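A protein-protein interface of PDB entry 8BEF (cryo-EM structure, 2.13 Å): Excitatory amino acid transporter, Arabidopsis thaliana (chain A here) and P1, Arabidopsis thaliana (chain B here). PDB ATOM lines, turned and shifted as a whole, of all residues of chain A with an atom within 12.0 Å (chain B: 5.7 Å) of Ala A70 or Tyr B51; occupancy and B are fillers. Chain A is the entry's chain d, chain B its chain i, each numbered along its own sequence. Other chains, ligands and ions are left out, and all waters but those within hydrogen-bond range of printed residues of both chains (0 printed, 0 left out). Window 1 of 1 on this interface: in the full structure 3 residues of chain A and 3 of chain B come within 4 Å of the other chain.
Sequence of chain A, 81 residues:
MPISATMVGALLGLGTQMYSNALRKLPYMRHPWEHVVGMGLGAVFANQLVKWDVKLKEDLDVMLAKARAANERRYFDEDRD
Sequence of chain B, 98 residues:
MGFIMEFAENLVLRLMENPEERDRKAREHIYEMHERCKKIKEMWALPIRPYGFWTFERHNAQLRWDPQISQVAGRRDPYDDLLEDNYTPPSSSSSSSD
The guanidinium group (NH2) of Arg A74 sits at hydrogen-bond distance from the side-chain amide oxygen (OD1) of Asn A71.
Among the printed residues, merely in contact across the chains: Ala A70 with Tyr B51 (3.9 Å), Ala A70 with Phe B56 (3.7 Å), Asn A71 with Pro B47 (3.2 Å), Arg A74 with Pro B47 (3.5 Å) and Arg A74 with Tyr B51 (3.4 Å).
Ala A70 touches just these residues of chain B: Tyr B51 and Phe B56.
Printed residues of chain B within 4 Å of Asn A71: Pro B47 (3.2 Å).
Of the printed residues of chain B, Arg A74 touches Pro B47 (3.5 Å) and Tyr B51 (3.4 Å).
No residue of chain A comes within 4 Å of Pro B50.
Of chain A, only Ala A70 (3.9 Å) and Arg A74 (3.4 Å) come within 4 Å of Tyr B51.
The nearest residue of chain B that does not touch Ala A70 is Pro B50 (4.6 Å).
The nearest printed residue of chain B that does not touch Arg A74 is Arg B49 (4.9 Å).
Hydrophobic or aromatic side chains of chain B that line the printed part of chain A: Pro B47, Tyr B51 and Phe B56.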
ATOM      1  N   ASP A  61      28.419  -7.069   9.206  1.00  0.00           N
ATOM      2  CA  ASP A  61      27.717  -7.629   8.053  1.00  0.00           C
ATOM      3  C   ASP A  61      27.306  -9.076   8.298  1.00  0.00           C
ATOM      4  O   ASP A  61      26.135  -9.435   8.135  1.00  0.00           O
ATOM      5  CB  ASP A  61      28.594  -7.521   6.809  1.00  0.00           C
ATOM      6  CG  ASP A  61      28.650  -6.112   6.267  1.00  0.00           C
ATOM      7  OD1 ASP A  61      27.771  -5.307   6.631  1.00  0.00           O
ATOM      8  OD2 ASP A  61      29.575  -5.807   5.485  1.00  0.00           O
ATOM      9  N   VAL A  62      28.259  -9.918   8.703  1.00  0.00           N
ATOM     10  CA  VAL A  62      27.956 -11.321   8.969  1.00  0.00           C
ATOM     11  C   VAL A  62      26.935 -11.444  10.090  1.00  0.00           C
ATOM     12  O   VAL A  62      26.046 -12.308  10.059  1.00  0.00           O
ATOM     13  CB  VAL A  62      29.245 -12.093   9.306  1.00  0.00           C
ATOM     14  CG1 VAL A  62      28.987 -13.587   9.271  1.00  0.00           C
ATOM     15  CG2 VAL A  62      30.366 -11.703   8.359  1.00  0.00           C
ATOM     16  N   MET A  63      27.052 -10.591  11.106  1.00  0.00           N
ATOM     17  CA  MET A  63      26.174 -10.739  12.259  1.00  0.00           C
ATOM     18  C   MET A  63      24.737 -10.359  11.904  1.00  0.00           C
ATOM     19  O   MET A  63      23.784 -11.037  12.313  1.00  0.00           O
ATOM     20  CB  MET A  63      26.722  -9.897  13.401  1.00  0.00           C
ATOM     21  CG  MET A  63      27.197 -10.731  14.563  1.00  0.00           C
ATOM     22  SD  MET A  63      27.757  -9.715  15.925  1.00  0.00           S
ATOM     23  CE  MET A  63      26.220  -9.562  16.786  1.00  0.00           C
ATOM     24  N   LEU A  64      24.569  -9.290  11.118  1.00  0.00           N
ATOM     25  CA  LEU A  64      23.256  -8.949  10.581  1.00  0.00           C
ATOM     26  C   LEU A  64      22.731 -10.045   9.665  1.00  0.00           C
ATOM     27  O   LEU A  64      21.525 -10.297   9.621  1.00  0.00           O
ATOM     28  CB  LEU A  64      23.323  -7.619   9.829  1.00  0.00           C
ATOM     29  CG  LEU A  64      23.507  -6.337  10.640  1.00  0.00           C
ATOM     30  CD1 LEU A  64      23.953  -5.200   9.746  1.00  0.00           C
ATOM     31  CD2 LEU A  64      22.204  -5.980  11.325  1.00  0.00           C
ATOM     32  N   ALA A  65      23.620 -10.698   8.913  1.00  0.00           N
ATOM     33  CA  ALA A  65      23.187 -11.806   8.065  1.00  0.00           C
ATOM     34  C   ALA A  65      22.582 -12.925   8.901  1.00  0.00           C
ATOM     35  O   ALA A  65      21.525 -13.473   8.563  1.00  0.00           O
ATOM     36  CB  ALA A  65      24.364 -12.331   7.241  1.00  0.00           C
ATOM     37  N   LYS A  66      23.245 -13.276  10.003  1.00  0.00           N
ATOM     38  CA  LYS A  66      22.718 -14.325  10.872  1.00  0.00           C
ATOM     39  C   LYS A  66      21.402 -13.904  11.514  1.00  0.00           C
ATOM     40  O   LYS A  66      20.472 -14.713  11.625  1.00  0.00           O
ATOM     41  CB  LYS A  66      23.739 -14.699  11.942  1.00  0.00           C
ATOM     42  CG  LYS A  66      24.985 -15.373  11.397  1.00  0.00           C
ATOM     43  CD  LYS A  66      25.995 -15.713  12.487  1.00  0.00           C
ATOM     44  CE  LYS A  66      27.231 -16.408  11.942  1.00  0.00           C
ATOM     45  NZ  LYS A  66      28.205 -16.704  13.025  1.00  0.00           N
ATOM     46  N   ALA A  67      21.306 -12.645  11.951  1.00  0.00           N
ATOM     47  CA  ALA A  67      20.043 -12.161  12.502  1.00  0.00           C
ATOM     48  C   ALA A  67      18.920 -12.269  11.476  1.00  0.00           C
ATOM     49  O   ALA A  67      17.810 -12.712  11.801  1.00  0.00           O
ATOM     50  CB  ALA A  67      20.195 -10.721  12.985  1.00  0.00           C
ATOM     51  N   ARG A  68      19.195 -11.874  10.230  1.00  0.00           N
ATOM     52  CA  ARG A  68      18.190 -11.951   9.176  1.00  0.00           C
ATOM     53  C   ARG A  68      17.772 -13.390   8.908  1.00  0.00           C
ATOM     54  O   ARG A  68      16.588 -13.666   8.699  1.00  0.00           O
ATOM     55  CB  ARG A  68      18.719 -11.313   7.893  1.00  0.00           C
ATOM     56  CG  ARG A  68      18.156  -9.934   7.599  1.00  0.00           C
ATOM     57  CD  ARG A  68      18.984  -9.235   6.536  1.00  0.00           C
ATOM     58  NE  ARG A  68      20.340  -8.963   6.999  1.00  0.00           N
ATOM     59  CZ  ARG A  68      21.407  -8.928   6.211  1.00  0.00           C
ATOM     60  NH1 ARG A  68      21.314  -9.150   4.911  1.00  0.00           N
ATOM     61  NH2 ARG A  68      22.597  -8.666   6.742  1.00  0.00           N
ATOM     62  N   ALA A  69      18.735 -14.315   8.878  1.00  0.00           N
ATOM     63  CA  ALA A  69      18.395 -15.720   8.667  1.00  0.00           C
ATOM     64  C   ALA A  69      17.516 -16.249   9.792  1.00  0.00           C
ATOM     65  O   ALA A  69      16.522 -16.949   9.545  1.00  0.00           O
ATOM     66  CB  ALA A  69      19.666 -16.559   8.550  1.00  0.00           C
ATOM     67  N   ALA A  70      17.866 -15.924  11.039  1.00  0.00           N
ATOM     68  CA  ALA A  70      17.064 -16.376  12.168  1.00  0.00           C
ATOM     69  C   ALA A  70      15.650 -15.819  12.092  1.00  0.00           C
ATOM     70  O   ALA A  70      14.680 -16.523  12.389  1.00  0.00           O
ATOM     71  CB  ALA A  70      17.731 -15.974  13.483  1.00  0.00           C
ATOM     72  N   ASN A  71      15.516 -14.549  11.699  1.00  0.00           N
ATOM     73  CA  ASN A  71      14.187 -13.964  11.547  1.00  0.00           C
ATOM     74  C   ASN A  71      13.406 -14.632  10.422  1.00  0.00           C
ATOM     75  O   ASN A  71      12.211 -14.916  10.572  1.00  0.00           O
ATOM     76  CB  ASN A  71      14.303 -12.461  11.298  1.00  0.00           C
ATOM     77  CG  ASN A  71      12.964 -11.758  11.355  1.00  0.00           C
ATOM     78  OD1 ASN A  71      12.208 -11.917  12.312  1.00  0.00           O
ATOM     79  ND2 ASN A  71      12.662 -10.976  10.326  1.00  0.00           N
ATOM     80  N   GLU A  72      14.061 -14.889   9.287  1.00  0.00           N
ATOM     81  CA  GLU A  72      13.393 -15.504   8.147  1.00  0.00           C
ATOM     82  C   GLU A  72      12.983 -16.940   8.427  1.00  0.00           C
ATOM     83  O   GLU A  72      12.081 -17.457   7.758  1.00  0.00           O
ATOM     84  CB  GLU A  72      14.300 -15.456   6.917  1.00  0.00           C
ATOM     85  CG  GLU A  72      14.556 -14.057   6.387  1.00  0.00           C
ATOM     86  CD  GLU A  72      15.516 -14.048   5.214  1.00  0.00           C
ATOM     87  OE1 GLU A  72      16.125 -15.104   4.937  1.00  0.00           O
ATOM     88  OE2 GLU A  72      15.662 -12.990   4.570  1.00  0.00           O
ATOM     89  N   ARG A  73      13.630 -17.598   9.392  1.00  0.00           N
ATOM     90  CA  ARG A  73      13.206 -18.939   9.777  1.00  0.00           C
ATOM     91  C   ARG A  73      11.778 -18.968  10.313  1.00  0.00           C
ATOM     92  O   ARG A  73      11.169 -20.043  10.360  1.00  0.00           O
ATOM     93  CB  ARG A  73      14.163 -19.518  10.819  1.00  0.00           C
ATOM     94  CG  ARG A  73      15.491 -19.982  10.247  1.00  0.00           C
ATOM     95  CD  ARG A  73      15.288 -21.043   9.180  1.00  0.00           C
ATOM     96  NE  ARG A  73      14.914 -22.331   9.753  1.00  0.00           N
ATOM     97  CZ  ARG A  73      15.774 -23.204  10.258  1.00  0.00           C
ATOM     98  NH1 ARG A  73      17.075 -22.962  10.274  1.00  0.00           N
ATOM     99  NH2 ARG A  73      15.319 -24.350  10.756  1.00  0.00           N
ATOM    100  N   ARG A  74      11.233 -17.818  10.724  1.00  0.00           N
ATOM    101  CA  ARG A  74       9.875 -17.788  11.262  1.00  0.00           C
ATOM    102  C   ARG A  74       8.842 -18.168  10.208  1.00  0.00           C
ATOM    103  O   ARG A  74       7.881 -18.889  10.504  1.00  0.00           O
ATOM    104  CB  ARG A  74       9.563 -16.404  11.834  1.00  0.00           C
ATOM    105  CG  ARG A  74       8.512 -16.424  12.932  1.00  0.00           C
ATOM    106  CD  ARG A  74       8.087 -15.026  13.348  1.00  0.00           C
ATOM    107  NE  ARG A  74       9.147 -14.309  14.047  1.00  0.00           N
ATOM    108  CZ  ARG A  74       9.765 -13.236  13.575  1.00  0.00           C
ATOM    109  NH1 ARG A  74       9.447 -12.716  12.402  1.00  0.00           N
ATOM    110  NH2 ARG A  74      10.722 -12.666  14.302  1.00  0.00           N
ATOM    111  N   TYR A  75       9.016 -17.692   8.977  1.00  0.00           N
ATOM    112  CA  TYR A  75       8.035 -17.889   7.919  1.00  0.00           C
ATOM    113  C   TYR A  75       8.201 -19.223   7.199  1.00  0.00           C
ATOM    114  O   TYR A  75       7.714 -19.376   6.074  1.00  0.00           O
ATOM    115  CB  TYR A  75       8.107 -16.734   6.920  1.00  0.00           C
ATOM    116  CG  TYR A  75       7.957 -15.372   7.562  1.00  0.00           C
ATOM    117  CD1 TYR A  75       7.015 -15.155   8.560  1.00  0.00           C
ATOM    118  CD2 TYR A  75       8.758 -14.307   7.175  1.00  0.00           C
ATOM    119  CE1 TYR A  75       6.873 -13.916   9.151  1.00  0.00           C
ATOM    120  CE2 TYR A  75       8.623 -13.063   7.761  1.00  0.00           C
ATOM    121  CZ  TYR A  75       7.679 -12.872   8.749  1.00  0.00           C
ATOM    122  OH  TYR A  75       7.540 -11.636   9.336  1.00  0.00           O
ATOM    123  N   PHE A  76       8.872 -20.188   7.821  1.00  0.00           N
ATOM    124  CA  PHE A  76       9.041 -21.509   7.231  1.00  0.00           C
ATOM    125  C   PHE A  76       7.940 -22.456   7.696  1.00  0.00           C
ATOM    126  O   PHE A  76       7.619 -22.512   8.884  1.00  0.00           O
ATOM    127  CB  PHE A  76      10.413 -22.083   7.585  1.00  0.00           C
ATOM    128  CG  PHE A  76      11.440 -21.906   6.505  1.00  0.00           C
ATOM    129  CD1 PHE A  76      11.594 -22.861   5.514  1.00  0.00           C
ATOM    130  CD2 PHE A  76      12.248 -20.782   6.477  1.00  0.00           C
ATOM    131  CE1 PHE A  76      12.538 -22.700   4.517  1.00  0.00           C
ATOM    132  CE2 PHE A  76      13.193 -20.616   5.483  1.00  0.00           C
ATOM    133  CZ  PHE A  76      13.338 -21.576   4.502  1.00  0.00           C
ATOM    134  N   PRO B  47      13.388  -7.868  14.745  1.00  0.00           N
ATOM    135  CA  PRO B  47      13.016  -8.130  16.141  1.00  0.00           C
ATOM    136  C   PRO B  47      14.228  -8.085  17.058  1.00  0.00           C
ATOM    137  O   PRO B  47      15.294  -8.615  16.738  1.00  0.00           O
ATOM    138  CB  PRO B  47      12.401  -9.533  16.082  1.00  0.00           C
ATOM    139  CG  PRO B  47      13.032 -10.158  14.886  1.00  0.00           C
ATOM    140  CD  PRO B  47      13.155  -9.043  13.889  1.00  0.00           C
ATOM    141  N   ARG B  49      14.182  -9.587  19.929  1.00  0.00           N
ATOM    142  CA  ARG B  49      14.190 -10.964  20.402  1.00  0.00           C
ATOM    143  C   ARG B  49      13.969 -11.875  19.204  1.00  0.00           C
ATOM    144  O   ARG B  49      12.830 -12.010  18.728  1.00  0.00           O
ATOM    145  CB  ARG B  49      13.096 -11.166  21.456  1.00  0.00           C
ATOM    146  CG  ARG B  49      13.161 -12.464  22.239  1.00  0.00           C
ATOM    147  CD  ARG B  49      12.351 -13.557  21.556  1.00  0.00           C
ATOM    148  NE  ARG B  49      10.938 -13.212  21.463  1.00  0.00           N
ATOM    149  CZ  ARG B  49      10.025 -13.955  20.851  1.00  0.00           C
ATOM    150  NH1 ARG B  49      10.343 -15.100  20.270  1.00  0.00           N
ATOM    151  NH2 ARG B  49       8.762 -13.540  20.824  1.00  0.00           N
ATOM    152  N   PRO B  50      15.057 -12.493  18.670  1.00  0.00           N
ATOM    153  CA  PRO B  50      14.893 -13.309  17.481  1.00  0.00           C
ATOM    154  C   PRO B  50      13.964 -14.511  17.713  1.00  0.00           C
ATOM    155  O   PRO B  50      13.680 -14.818  18.844  1.00  0.00           O
ATOM    156  CB  PRO B  50      16.365 -13.655  17.157  1.00  0.00           C
ATOM    157  CG  PRO B  50      17.077 -13.657  18.452  1.00  0.00           C
ATOM    158  CD  PRO B  50      16.462 -12.469  19.131  1.00  0.00           C
ATOM    159  N   TYR B  51      13.496 -15.137  16.660  1.00  0.00           N
ATOM    160  CA  TYR B  51      12.669 -16.333  16.734  1.00  0.00           C
ATOM    161  C   TYR B  51      13.471 -17.498  17.297  1.00  0.00           C
ATOM    162  O   TYR B  51      14.445 -17.946  16.685  1.00  0.00           O
ATOM    163  CB  TYR B  51      12.141 -16.671  15.342  1.00  0.00           C
ATOM    164  CG  TYR B  51      10.944 -17.595  15.311  1.00  0.00           C
ATOM    165  CD1 TYR B  51       9.876 -17.416  16.176  1.00  0.00           C
ATOM    166  CD2 TYR B  51      10.884 -18.644  14.405  1.00  0.00           C
ATOM    167  CE1 TYR B  51       8.781 -18.258  16.140  1.00  0.00           C
ATOM    168  CE2 TYR B  51       9.798 -19.488  14.360  1.00  0.00           C
ATOM    169  CZ  TYR B  51       8.748 -19.291  15.228  1.00  0.00           C
ATOM    170  OH  TYR B  51       7.666 -20.136  15.181  1.00  0.00           O
ATOM    171  N   GLY B  52      13.056 -17.991  18.462  1.00  0.00           N
ATOM    172  CA  GLY B  52      13.695 -19.142  19.068  1.00  0.00           C
ATOM    173  C   GLY B  52      15.159 -18.934  19.390  1.00  0.00           C
ATOM    174  O   GLY B  52      15.995 -19.763  19.029  1.00  0.00           O
ATOM    175  N   PHE B  53      15.489 -17.822  20.052  1.00  0.00           N
ATOM    176  CA  PHE B  53      16.890 -17.547  20.356  1.00  0.00           C
ATOM    177  C   PHE B  53      17.479 -18.625  21.259  1.00  0.00           C
ATOM    178  O   PHE B  53      18.642 -19.008  21.100  1.00  0.00           O
ATOM    179  CB  PHE B  53      17.038 -16.168  20.996  1.00  0.00           C
ATOM    180  CG  PHE B  53      16.308 -16.017  22.299  1.00  0.00           C
ATOM    181  CD1 PHE B  53      14.971 -15.663  22.325  1.00  0.00           C
ATOM    182  CD2 PHE B  53      16.962 -16.219  23.502  1.00  0.00           C
ATOM    183  CE1 PHE B  53      14.303 -15.522  23.526  1.00  0.00           C
ATOM    184  CE2 PHE B  53      16.296 -16.081  24.701  1.00  0.00           C
ATOM    185  CZ  PHE B  53      14.970 -15.731  24.715  1.00  0.00           C
ATOM    186  N   TRP B  54      16.681 -19.148  22.193  1.00  0.00           N
ATOM    187  CA  TRP B  54      17.144 -20.195  23.095  1.00  0.00           C
ATOM    188  C   TRP B  54      17.499 -21.486  22.367  1.00  0.00           C
ATOM    189  O   TRP B  54      18.131 -22.361  22.968  1.00  0.00           O
ATOM    190  CB  TRP B  54      16.081 -20.464  24.163  1.00  0.00           C
ATOM    191  CG  TRP B  54      14.794 -20.929  23.577  1.00  0.00           C
ATOM    192  CD1 TRP B  54      14.441 -22.208  23.302  1.00  0.00           C
ATOM    193  CD2 TRP B  54      13.697 -20.109  23.160  1.00  0.00           C
ATOM    194  NE1 TRP B  54      13.185 -22.245  22.746  1.00  0.00           N
ATOM    195  CE2 TRP B  54      12.706 -20.967  22.648  1.00  0.00           C
ATOM    196  CE3 TRP B  54      13.455 -18.734  23.173  1.00  0.00           C
ATOM    197  CZ2 TRP B  54      11.491 -20.496  22.161  1.00  0.00           C
ATOM    198  CZ3 TRP B  54      12.249 -18.267  22.686  1.00  0.00           C
ATOM    199  CH2 TRP B  54      11.282 -19.146  22.187  1.00  0.00           C
ATOM    200  N   PHE B  56      19.543 -21.366  19.773  1.00  0.00           N
ATOM    201  CA  PHE B  56      20.909 -21.085  19.296  1.00  0.00           C
ATOM    202  C   PHE B  56      21.944 -21.800  20.197  1.00  0.00           C
ATOM    203  O   PHE B  56      21.795 -21.740  21.431  1.00  0.00           O
ATOM    204  CB  PHE B  56      21.103 -19.583  19.149  1.00  0.00           C
ATOM    205  CG  PHE B  56      20.112 -18.800  18.327  1.00  0.00           C
ATOM    206  CD1 PHE B  56      19.322 -19.402  17.365  1.00  0.00           C
ATOM    207  CD2 PHE B  56      19.973 -17.436  18.528  1.00  0.00           C
ATOM    208  CE1 PHE B  56      18.410 -18.663  16.633  1.00  0.00           C
ATOM    209  CE2 PHE B  56      19.049 -16.698  17.804  1.00  0.00           C
ATOM    210  CZ  PHE B  56      18.275 -17.316  16.855  1.00  0.00           C
